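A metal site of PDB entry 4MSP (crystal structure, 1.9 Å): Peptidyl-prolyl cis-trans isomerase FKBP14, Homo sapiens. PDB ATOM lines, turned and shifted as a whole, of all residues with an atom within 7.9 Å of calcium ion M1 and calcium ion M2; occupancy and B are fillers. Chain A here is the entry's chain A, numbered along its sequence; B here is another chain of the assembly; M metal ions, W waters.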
ATOM      1  N   ARG A 128      24.757  -5.833  22.543  1.00  0.00           N
ATOM      2  CA  ARG A 128      25.213  -4.871  21.547  1.00  0.00           C
ATOM      3  C   ARG A 128      26.197  -5.566  20.618  1.00  0.00           C
ATOM      4  O   ARG A 128      27.155  -6.157  21.096  1.00  0.00           O
ATOM      5  CB  ARG A 128      25.908  -3.675  22.208  1.00  0.00           C
ATOM      6  CG  ARG A 128      24.986  -2.715  22.963  1.00  0.00           C
ATOM      7  CD  ARG A 128      25.163  -1.298  22.453  1.00  0.00           C
ATOM      8  NE  ARG A 128      24.227  -0.358  23.053  1.00  0.00           N
ATOM      9  CZ  ARG A 128      24.569   0.638  23.865  1.00  0.00           C
ATOM     10  NH1 ARG A 128      25.856   0.829  24.183  1.00  0.00           N
ATOM     11  NH2 ARG A 128      23.643   1.456  24.362  1.00  0.00           N
ATOM     12  N   LYS A 143      33.007   6.107  15.181  1.00  0.00           N
ATOM     13  CA  LYS A 143      32.132   6.739  16.169  1.00  0.00           C
ATOM     14  C   LYS A 143      30.808   7.104  15.513  1.00  0.00           C
ATOM     15  O   LYS A 143      30.720   7.283  14.296  1.00  0.00           O
ATOM     16  CB  LYS A 143      32.801   7.957  16.828  1.00  0.00           C
ATOM     17  CG  LYS A 143      33.065   9.119  15.898  1.00  0.00           C
ATOM     18  CD  LYS A 143      34.119  10.061  16.478  1.00  0.00           C
ATOM     19  CE  LYS A 143      34.462  11.158  15.494  1.00  0.00           C
ATOM     20  NZ  LYS A 143      35.655  11.957  15.914  1.00  0.00           N
ATOM     21  N   LEU A 144      29.761   7.186  16.338  1.00  0.00           N
ATOM     22  CA  LEU A 144      28.429   7.472  15.819  1.00  0.00           C
ATOM     23  C   LEU A 144      28.077   8.919  16.101  1.00  0.00           C
ATOM     24  O   LEU A 144      28.037   9.328  17.262  1.00  0.00           O
ATOM     25  CB  LEU A 144      27.412   6.573  16.513  1.00  0.00           C
ATOM     26  CG  LEU A 144      27.769   5.087  16.548  1.00  0.00           C
ATOM     27  CD1 LEU A 144      26.658   4.288  17.201  1.00  0.00           C
ATOM     28  CD2 LEU A 144      28.036   4.586  15.145  1.00  0.00           C
ATOM     29  N   PHE A 177      22.222  10.067  23.705  1.00  0.00           N
ATOM     30  CA  PHE A 177      23.570  10.598  23.883  1.00  0.00           C
ATOM     31  C   PHE A 177      23.840  11.056  25.314  1.00  0.00           C
ATOM     32  O   PHE A 177      24.991  11.078  25.755  1.00  0.00           O
ATOM     33  CB  PHE A 177      23.874  11.720  22.891  1.00  0.00           C
ATOM     34  CG  PHE A 177      24.348  11.229  21.547  1.00  0.00           C
ATOM     35  CD1 PHE A 177      25.630  11.512  21.104  1.00  0.00           C
ATOM     36  CD2 PHE A 177      23.503  10.496  20.723  1.00  0.00           C
ATOM     37  CE1 PHE A 177      26.074  11.055  19.866  1.00  0.00           C
ATOM     38  CE2 PHE A 177      23.937  10.038  19.487  1.00  0.00           C
ATOM     39  CZ  PHE A 177      25.222  10.316  19.052  1.00  0.00           C
ATOM     40  N   LYS A 179      23.316   9.521  27.933  1.00  0.00           N
ATOM     41  CA  LYS A 179      23.938   8.386  28.612  1.00  0.00           C
ATOM     42  C   LYS A 179      25.206   7.869  27.920  1.00  0.00           C
ATOM     43  O   LYS A 179      26.186   7.553  28.586  1.00  0.00           O
ATOM     44  CB  LYS A 179      22.941   7.231  28.749  1.00  0.00           C
ATOM     45  CG  LYS A 179      21.935   7.413  29.867  1.00  0.00           C
ATOM     46  CD  LYS A 179      21.096   6.152  30.045  1.00  0.00           C
ATOM     47  CE  LYS A 179      21.972   4.921  30.275  1.00  0.00           C
ATOM     48  NZ  LYS A 179      21.163   3.690  30.486  1.00  0.00           N
ATOM     49  N   GLU A 180      25.183   7.776  26.597  1.00  0.00           N
ATOM     50  CA  GLU A 180      26.223   7.057  25.880  1.00  0.00           C
ATOM     51  C   GLU A 180      27.430   7.894  25.512  1.00  0.00           C
ATOM     52  O   GLU A 180      28.537   7.360  25.401  1.00  0.00           O
ATOM     53  CB  GLU A 180      25.641   6.376  24.621  1.00  0.00           C
ATOM     54  CG  GLU A 180      24.501   5.403  24.895  1.00  0.00           C
ATOM     55  CD  GLU A 180      24.961   4.110  25.565  1.00  0.00           C
ATOM     56  OE1 GLU A 180      26.151   3.775  25.477  1.00  0.00           O
ATOM     57  OE2 GLU A 180      24.105   3.432  26.172  1.00  0.00           O
ATOM     58  N   ASP A 181      27.233   9.188  25.306  1.00  0.00           N
ATOM     59  CA  ASP A 181      28.361  10.095  25.057  1.00  0.00           C
ATOM     60  C   ASP A 181      28.928  10.584  26.384  1.00  0.00           C
ATOM     61  O   ASP A 181      28.288  11.363  27.080  1.00  0.00           O
ATOM     62  CB  ASP A 181      27.924  11.282  24.203  1.00  0.00           C
ATOM     63  CG  ASP A 181      29.082  12.157  23.789  1.00  0.00           C
ATOM     64  OD1 ASP A 181      30.244  11.718  23.927  1.00  0.00           O
ATOM     65  OD2 ASP A 181      28.842  13.288  23.311  1.00  0.00           O
ATOM     66  N   GLU A 182      30.123  10.129  26.734  1.00  0.00           N
ATOM     67  CA  GLU A 182      30.685  10.415  28.059  1.00  0.00           C
ATOM     68  C   GLU A 182      31.626  11.605  28.060  1.00  0.00           C
ATOM     69  O   GLU A 182      31.510  12.490  28.905  1.00  0.00           O
ATOM     70  CB  GLU A 182      31.400   9.191  28.615  1.00  0.00           C
ATOM     71  CG  GLU A 182      30.480   8.025  28.927  1.00  0.00           C
ATOM     72  CD  GLU A 182      31.241   6.770  29.302  1.00  0.00           C
ATOM     73  OE1 GLU A 182      32.133   6.852  30.171  1.00  0.00           O
ATOM     74  OE2 GLU A 182      30.953   5.712  28.702  1.00  0.00           O
ATOM     75  N   ASP A 183      32.578  11.626  27.134  1.00  0.00           N
ATOM     76  CA  ASP A 183      33.476  12.784  27.032  1.00  0.00           C
ATOM     77  C   ASP A 183      32.774  13.991  26.412  1.00  0.00           C
ATOM     78  O   ASP A 183      33.316  15.101  26.410  1.00  0.00           O
ATOM     79  CB  ASP A 183      34.777  12.445  26.293  1.00  0.00           C
ATOM     80  CG  ASP A 183      34.552  11.769  24.944  1.00  0.00           C
ATOM     81  OD1 ASP A 183      35.556  11.340  24.345  1.00  0.00           O
ATOM     82  OD2 ASP A 183      33.390  11.662  24.503  1.00  0.00           O
ATOM     83  N   LYS A 184      31.565  13.759  25.897  1.00  0.00           N
ATOM     84  CA  LYS A 184      30.740  14.803  25.302  1.00  0.00           C
ATOM     85  C   LYS A 184      31.416  15.470  24.099  1.00  0.00           C
ATOM     86  O   LYS A 184      31.336  16.699  23.936  1.00  0.00           O
ATOM     87  CB  LYS A 184      30.334  15.862  26.327  1.00  0.00           C
ATOM     88  CG  LYS A 184      29.673  15.306  27.583  1.00  0.00           C
ATOM     89  CD  LYS A 184      28.455  14.459  27.251  1.00  0.00           C
ATOM     90  CE  LYS A 184      27.700  14.090  28.518  1.00  0.00           C
ATOM     91  NZ  LYS A 184      26.696  13.020  28.270  1.00  0.00           N
ATOM     92  N   ASP A 185      32.065  14.670  23.253  1.00  0.00           N
ATOM     93  CA  ASP A 185      32.586  15.204  22.006  1.00  0.00           C
ATOM     94  C   ASP A 185      31.486  15.236  20.946  1.00  0.00           C
ATOM     95  O   ASP A 185      31.694  15.695  19.829  1.00  0.00           O
ATOM     96  CB  ASP A 185      33.859  14.476  21.524  1.00  0.00           C
ATOM     97  CG  ASP A 185      33.603  13.018  21.154  1.00  0.00           C
ATOM     98  OD1 ASP A 185      32.638  12.416  21.661  1.00  0.00           O
ATOM     99  OD2 ASP A 185      34.410  12.475  20.366  1.00  0.00           O
ATOM    100  N   GLY A 186      30.304  14.751  21.329  1.00  0.00           N
ATOM    101  CA  GLY A 186      29.151  14.744  20.446  1.00  0.00           C
ATOM    102  C   GLY A 186      29.008  13.433  19.690  1.00  0.00           C
ATOM    103  O   GLY A 186      28.148  13.299  18.814  1.00  0.00           O
ATOM    104  N   PHE A 187      29.842  12.469  20.038  1.00  0.00           N
ATOM    105  CA  PHE A 187      29.856  11.181  19.366  1.00  0.00           C
ATOM    106  C   PHE A 187      29.766  10.034  20.359  1.00  0.00           C
ATOM    107  O   PHE A 187      30.030  10.195  21.546  1.00  0.00           O
ATOM    108  CB  PHE A 187      31.134  11.005  18.541  1.00  0.00           C
ATOM    109  CG  PHE A 187      31.350  12.084  17.526  1.00  0.00           C
ATOM    110  CD1 PHE A 187      32.137  13.189  17.831  1.00  0.00           C
ATOM    111  CD2 PHE A 187      30.785  11.989  16.259  1.00  0.00           C
ATOM    112  CE1 PHE A 187      32.348  14.179  16.897  1.00  0.00           C
ATOM    113  CE2 PHE A 187      30.986  12.976  15.327  1.00  0.00           C
ATOM    114  CZ  PHE A 187      31.766  14.074  15.642  1.00  0.00           C
ATOM    115  N   ILE A 188      29.395   8.868  19.854  1.00  0.00           N
ATOM    116  CA  ILE A 188      29.462   7.648  20.639  1.00  0.00           C
ATOM    117  C   ILE A 188      30.545   6.774  20.018  1.00  0.00           C
ATOM    118  O   ILE A 188      30.316   6.110  18.996  1.00  0.00           O
ATOM    119  CB  ILE A 188      28.120   6.925  20.645  1.00  0.00           C
ATOM    120  CG1 ILE A 188      27.040   7.820  21.253  1.00  0.00           C
ATOM    121  CG2 ILE A 188      28.217   5.603  21.406  1.00  0.00           C
ATOM    122  CD1 ILE A 188      25.640   7.266  21.102  1.00  0.00           C
ATOM    123  N   SER A 189      31.726   6.799  20.622  1.00  0.00           N
ATOM    124  CA  SER A 189      32.861   5.999  20.153  1.00  0.00           C
ATOM    125  C   SER A 189      32.575   4.510  20.263  1.00  0.00           C
ATOM    126  O   SER A 189      31.644   4.089  20.958  1.00  0.00           O
ATOM    127  CB  SER A 189      34.090   6.317  20.997  1.00  0.00           C
ATOM    128  OG  SER A 189      33.888   5.856  22.317  1.00  0.00           O
ATOM    129  N   ALA A 190      33.381   3.704  19.581  1.00  0.00           N
ATOM    130  CA  ALA A 190      33.239   2.248  19.665  1.00  0.00           C
ATOM    131  C   ALA A 190      33.371   1.800  21.115  1.00  0.00           C
ATOM    132  O   ALA A 190      32.629   0.920  21.572  1.00  0.00           O
ATOM    133  CB  ALA A 190      34.275   1.557  18.794  1.00  0.00           C
ATOM    134  N   ARG A 191      34.297   2.412  21.826  1.00  0.00           N
ATOM    135  CA  ARG A 191      34.497   2.139  23.241  1.00  0.00           C
ATOM    136  C   ARG A 191      33.216   2.399  24.047  1.00  0.00           C
ATOM    137  O   ARG A 191      32.743   1.511  24.764  1.00  0.00           O
ATOM    138  CB  ARG A 191      35.661   2.975  23.780  1.00  0.00           C
ATOM    139  CG  ARG A 191      36.191   2.532  25.128  1.00  0.00           C
ATOM    140  CD  ARG A 191      37.621   2.991  25.319  1.00  0.00           C
ATOM    141  NE  ARG A 191      38.123   2.658  26.659  1.00  0.00           N
ATOM    142  CZ  ARG A 191      38.120   3.512  27.680  1.00  0.00           C
ATOM    143  NH1 ARG A 191      37.645   4.740  27.525  1.00  0.00           N
ATOM    144  NH2 ARG A 191      38.595   3.125  28.860  1.00  0.00           N
ATOM    145  N   GLU A 192      32.654   3.595  23.888  1.00  0.00           N
ATOM    146  CA  GLU A 192      31.411   3.953  24.570  1.00  0.00           C
ATOM    147  C   GLU A 192      30.236   3.028  24.200  1.00  0.00           C
ATOM    148  O   GLU A 192      29.383   2.739  25.037  1.00  0.00           O
ATOM    149  CB  GLU A 192      31.035   5.413  24.282  1.00  0.00           C
ATOM    150  CG  GLU A 192      31.870   6.442  25.037  1.00  0.00           C
ATOM    151  CD  GLU A 192      31.706   7.852  24.476  1.00  0.00           C
ATOM    152  OE1 GLU A 192      31.451   7.987  23.262  1.00  0.00           O
ATOM    153  OE2 GLU A 192      31.827   8.825  25.249  1.00  0.00           O
ATOM    154  N   PHE A 193      30.210   2.561  22.952  1.00  0.00           N
ATOM    155  CA  PHE A 193      29.117   1.698  22.483  1.00  0.00           C
ATOM    156  C   PHE A 193      29.155   0.295  23.102  1.00  0.00           C
ATOM    157  O   PHE A 193      28.105  -0.326  23.296  1.00  0.00           O
ATOM    158  CB  PHE A 193      29.165   1.582  20.952  1.00  0.00           C
ATOM    159  CG  PHE A 193      28.014   0.820  20.357  1.00  0.00           C
ATOM    160  CD1 PHE A 193      26.825   1.464  20.050  1.00  0.00           C
ATOM    161  CD2 PHE A 193      28.131  -0.530  20.053  1.00  0.00           C
ATOM    162  CE1 PHE A 193      25.764   0.775  19.470  1.00  0.00           C
ATOM    163  CE2 PHE A 193      27.076  -1.230  19.490  1.00  0.00           C
ATOM    164  CZ  PHE A 193      25.884  -0.570  19.193  1.00  0.00           C
ATOM    165  N   THR A 194      30.358  -0.189  23.406  1.00  0.00           N
ATOM    166  CA  THR A 194      30.586  -1.570  23.842  1.00  0.00           C
ATOM    167  C   THR A 194      29.641  -2.063  24.936  1.00  0.00           C
ATOM    168  O   THR A 194      28.935  -3.061  24.757  1.00  0.00           O
ATOM    169  CB  THR A 194      32.038  -1.771  24.326  1.00  0.00           C
ATOM    170  OG1 THR A 194      32.933  -1.497  23.246  1.00  0.00           O
ATOM    171  CG2 THR A 194      32.253  -3.200  24.797  1.00  0.00           C
ATOM    172  N   TYR A 195      29.611  -1.367  26.064  1.00  0.00           N
ATOM    173  CA  TYR A 195      28.704  -1.726  27.144  1.00  0.00           C
ATOM    174  C   TYR A 195      27.532  -0.760  27.227  1.00  0.00           C
ATOM    175  O   TYR A 195      27.722   0.454  27.209  1.00  0.00           O
ATOM    176  CB  TYR A 195      29.443  -1.732  28.486  1.00  0.00           C
ATOM    177  CG  TYR A 195      30.581  -2.735  28.562  1.00  0.00           C
ATOM    178  CD1 TYR A 195      31.875  -2.364  28.243  1.00  0.00           C
ATOM    179  CD2 TYR A 195      30.346  -4.051  28.947  1.00  0.00           C
ATOM    180  CE1 TYR A 195      32.920  -3.281  28.318  1.00  0.00           C
ATOM    181  CE2 TYR A 195      31.371  -4.964  29.031  1.00  0.00           C
ATOM    182  CZ  TYR A 195      32.658  -4.575  28.701  1.00  0.00           C
ATOM    183  OH  TYR A 195      33.689  -5.480  28.775  1.00  0.00           O
ATOM    184  N   LYS A 196      26.328  -1.314  27.293  1.00  0.00           N
ATOM    185  CA  LYS A 196      25.205  -0.511  27.723  1.00  0.00           C
ATOM    186  C   LYS A 196      25.518  -0.250  29.189  1.00  0.00           C
ATOM    187  O   LYS A 196      25.447  -1.172  30.008  1.00  0.00           O
ATOM    188  CB  LYS A 196      23.891  -1.290  27.636  1.00  0.00           C
ATOM    189  CG  LYS A 196      23.673  -2.078  26.349  1.00  0.00           C
ATOM    190  CD  LYS A 196      22.453  -2.987  26.493  1.00  0.00           C
ATOM    191  CE  LYS A 196      22.335  -3.995  25.355  1.00  0.00           C
ATOM    192  NZ  LYS A 196      21.282  -5.035  25.619  1.00  0.00           N
ATOM    193  N   HIS A 197      25.865   0.982  29.534  1.00  0.00           N
ATOM    194  CA  HIS A 197      26.152   1.296  30.931  1.00  0.00           C
ATOM    195  C   HIS A 197      24.866   1.327  31.755  1.00  0.00           C
ATOM    196  O   HIS A 197      24.859   1.696  32.928  1.00  0.00           O
ATOM    197  CB  HIS A 197      26.970   2.577  31.066  1.00  0.00           C
ATOM    198  CG  HIS A 197      28.398   2.432  30.639  1.00  0.00           C
ATOM    199  ND1 HIS A 197      28.841   2.799  29.375  1.00  0.00           N
ATOM    200  CD2 HIS A 197      29.488   1.941  31.281  1.00  0.00           C
ATOM    201  CE1 HIS A 197      30.136   2.543  29.277  1.00  0.00           C
ATOM    202  NE2 HIS A 197      30.548   2.033  30.413  1.00  0.00           N
ATOM    203  N   ASP A 198      23.775   0.927  31.096  1.00  0.00           N
ATOM    204  CA  ASP A 198      22.494   0.652  31.728  1.00  0.00           C
ATOM    205  C   ASP A 198      22.637  -0.525  32.698  1.00  0.00           C
ATOM    206  O   ASP A 198      23.235  -1.548  32.365  1.00  0.00           O
ATOM    207  CB  ASP A 198      21.463   0.333  30.647  1.00  0.00           C
ATOM    208  CG  ASP A 198      20.070   0.080  31.207  1.00  0.00           C
ATOM    209  OD1 ASP A 198      19.837   0.361  32.401  1.00  0.00           O
ATOM    210  OD2 ASP A 198      19.202  -0.378  30.439  1.00  0.00           O
ATOM    211  N   GLY B 161      19.806  -0.628  24.775  1.00  0.00           N
ATOM    212  CA  GLY B 161      20.333   0.043  25.948  1.00  0.00           C
ATOM    213  C   GLY B 161      20.137   1.552  25.851  1.00  0.00           C
ATOM    214  O   GLY B 161      20.892   2.321  26.458  1.00  0.00           O
HETATM  215 CA    CA M   1      31.989  10.544  22.999  1.00  0.00          CA
HETATM  216 CA    CA M   2      28.054   2.900  27.043  1.00  0.00          CA
HETATM  217  O   HOH W   1      33.911   9.995  21.337  1.00  0.00           O
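Calcium ion M1 is bound by the side-chain carboxylate (OD1) of Asp 181, the side-chain carboxylate (OD2) of Asp 183, the side-chain carboxylate (OD1) of Asp 185, the backbone carbonyl oxygen (O) of Phe 187, water W1, the side-chain carboxylate (OE1) of Glu 192 and the side-chain carboxylate (OE2) of Glu 192.
Calcium ion M2 is bound by O of Glu 192, ND1 of His 197, O of Tyr 195 and OE1 of Glu 180.
Of the 25 residues printed, 4 come within 4 Å of calcium ion M2.
N of Glu 182 lies close to OE2 of Glu 192, 2.6 Å away. O of Asp 181 lies within hydrogen-bond range of NZ of Lys 184 (2.6 Å). OD2 of Asp 181 lies within hydrogen-bond range of N of Gly 186 (2.9 Å). OE2 of Glu 180 is in salt-bridge range of NH2 of Arg 128 (2.7 Å). The backbone NH (N) of Glu 192 is in hydrogen-bond range of the side-chain hydroxyl (OG) of Ser 189, 3.0 Å away.
Of the 25 residues printed, 5 come within 4 Å of calcium ion M1.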
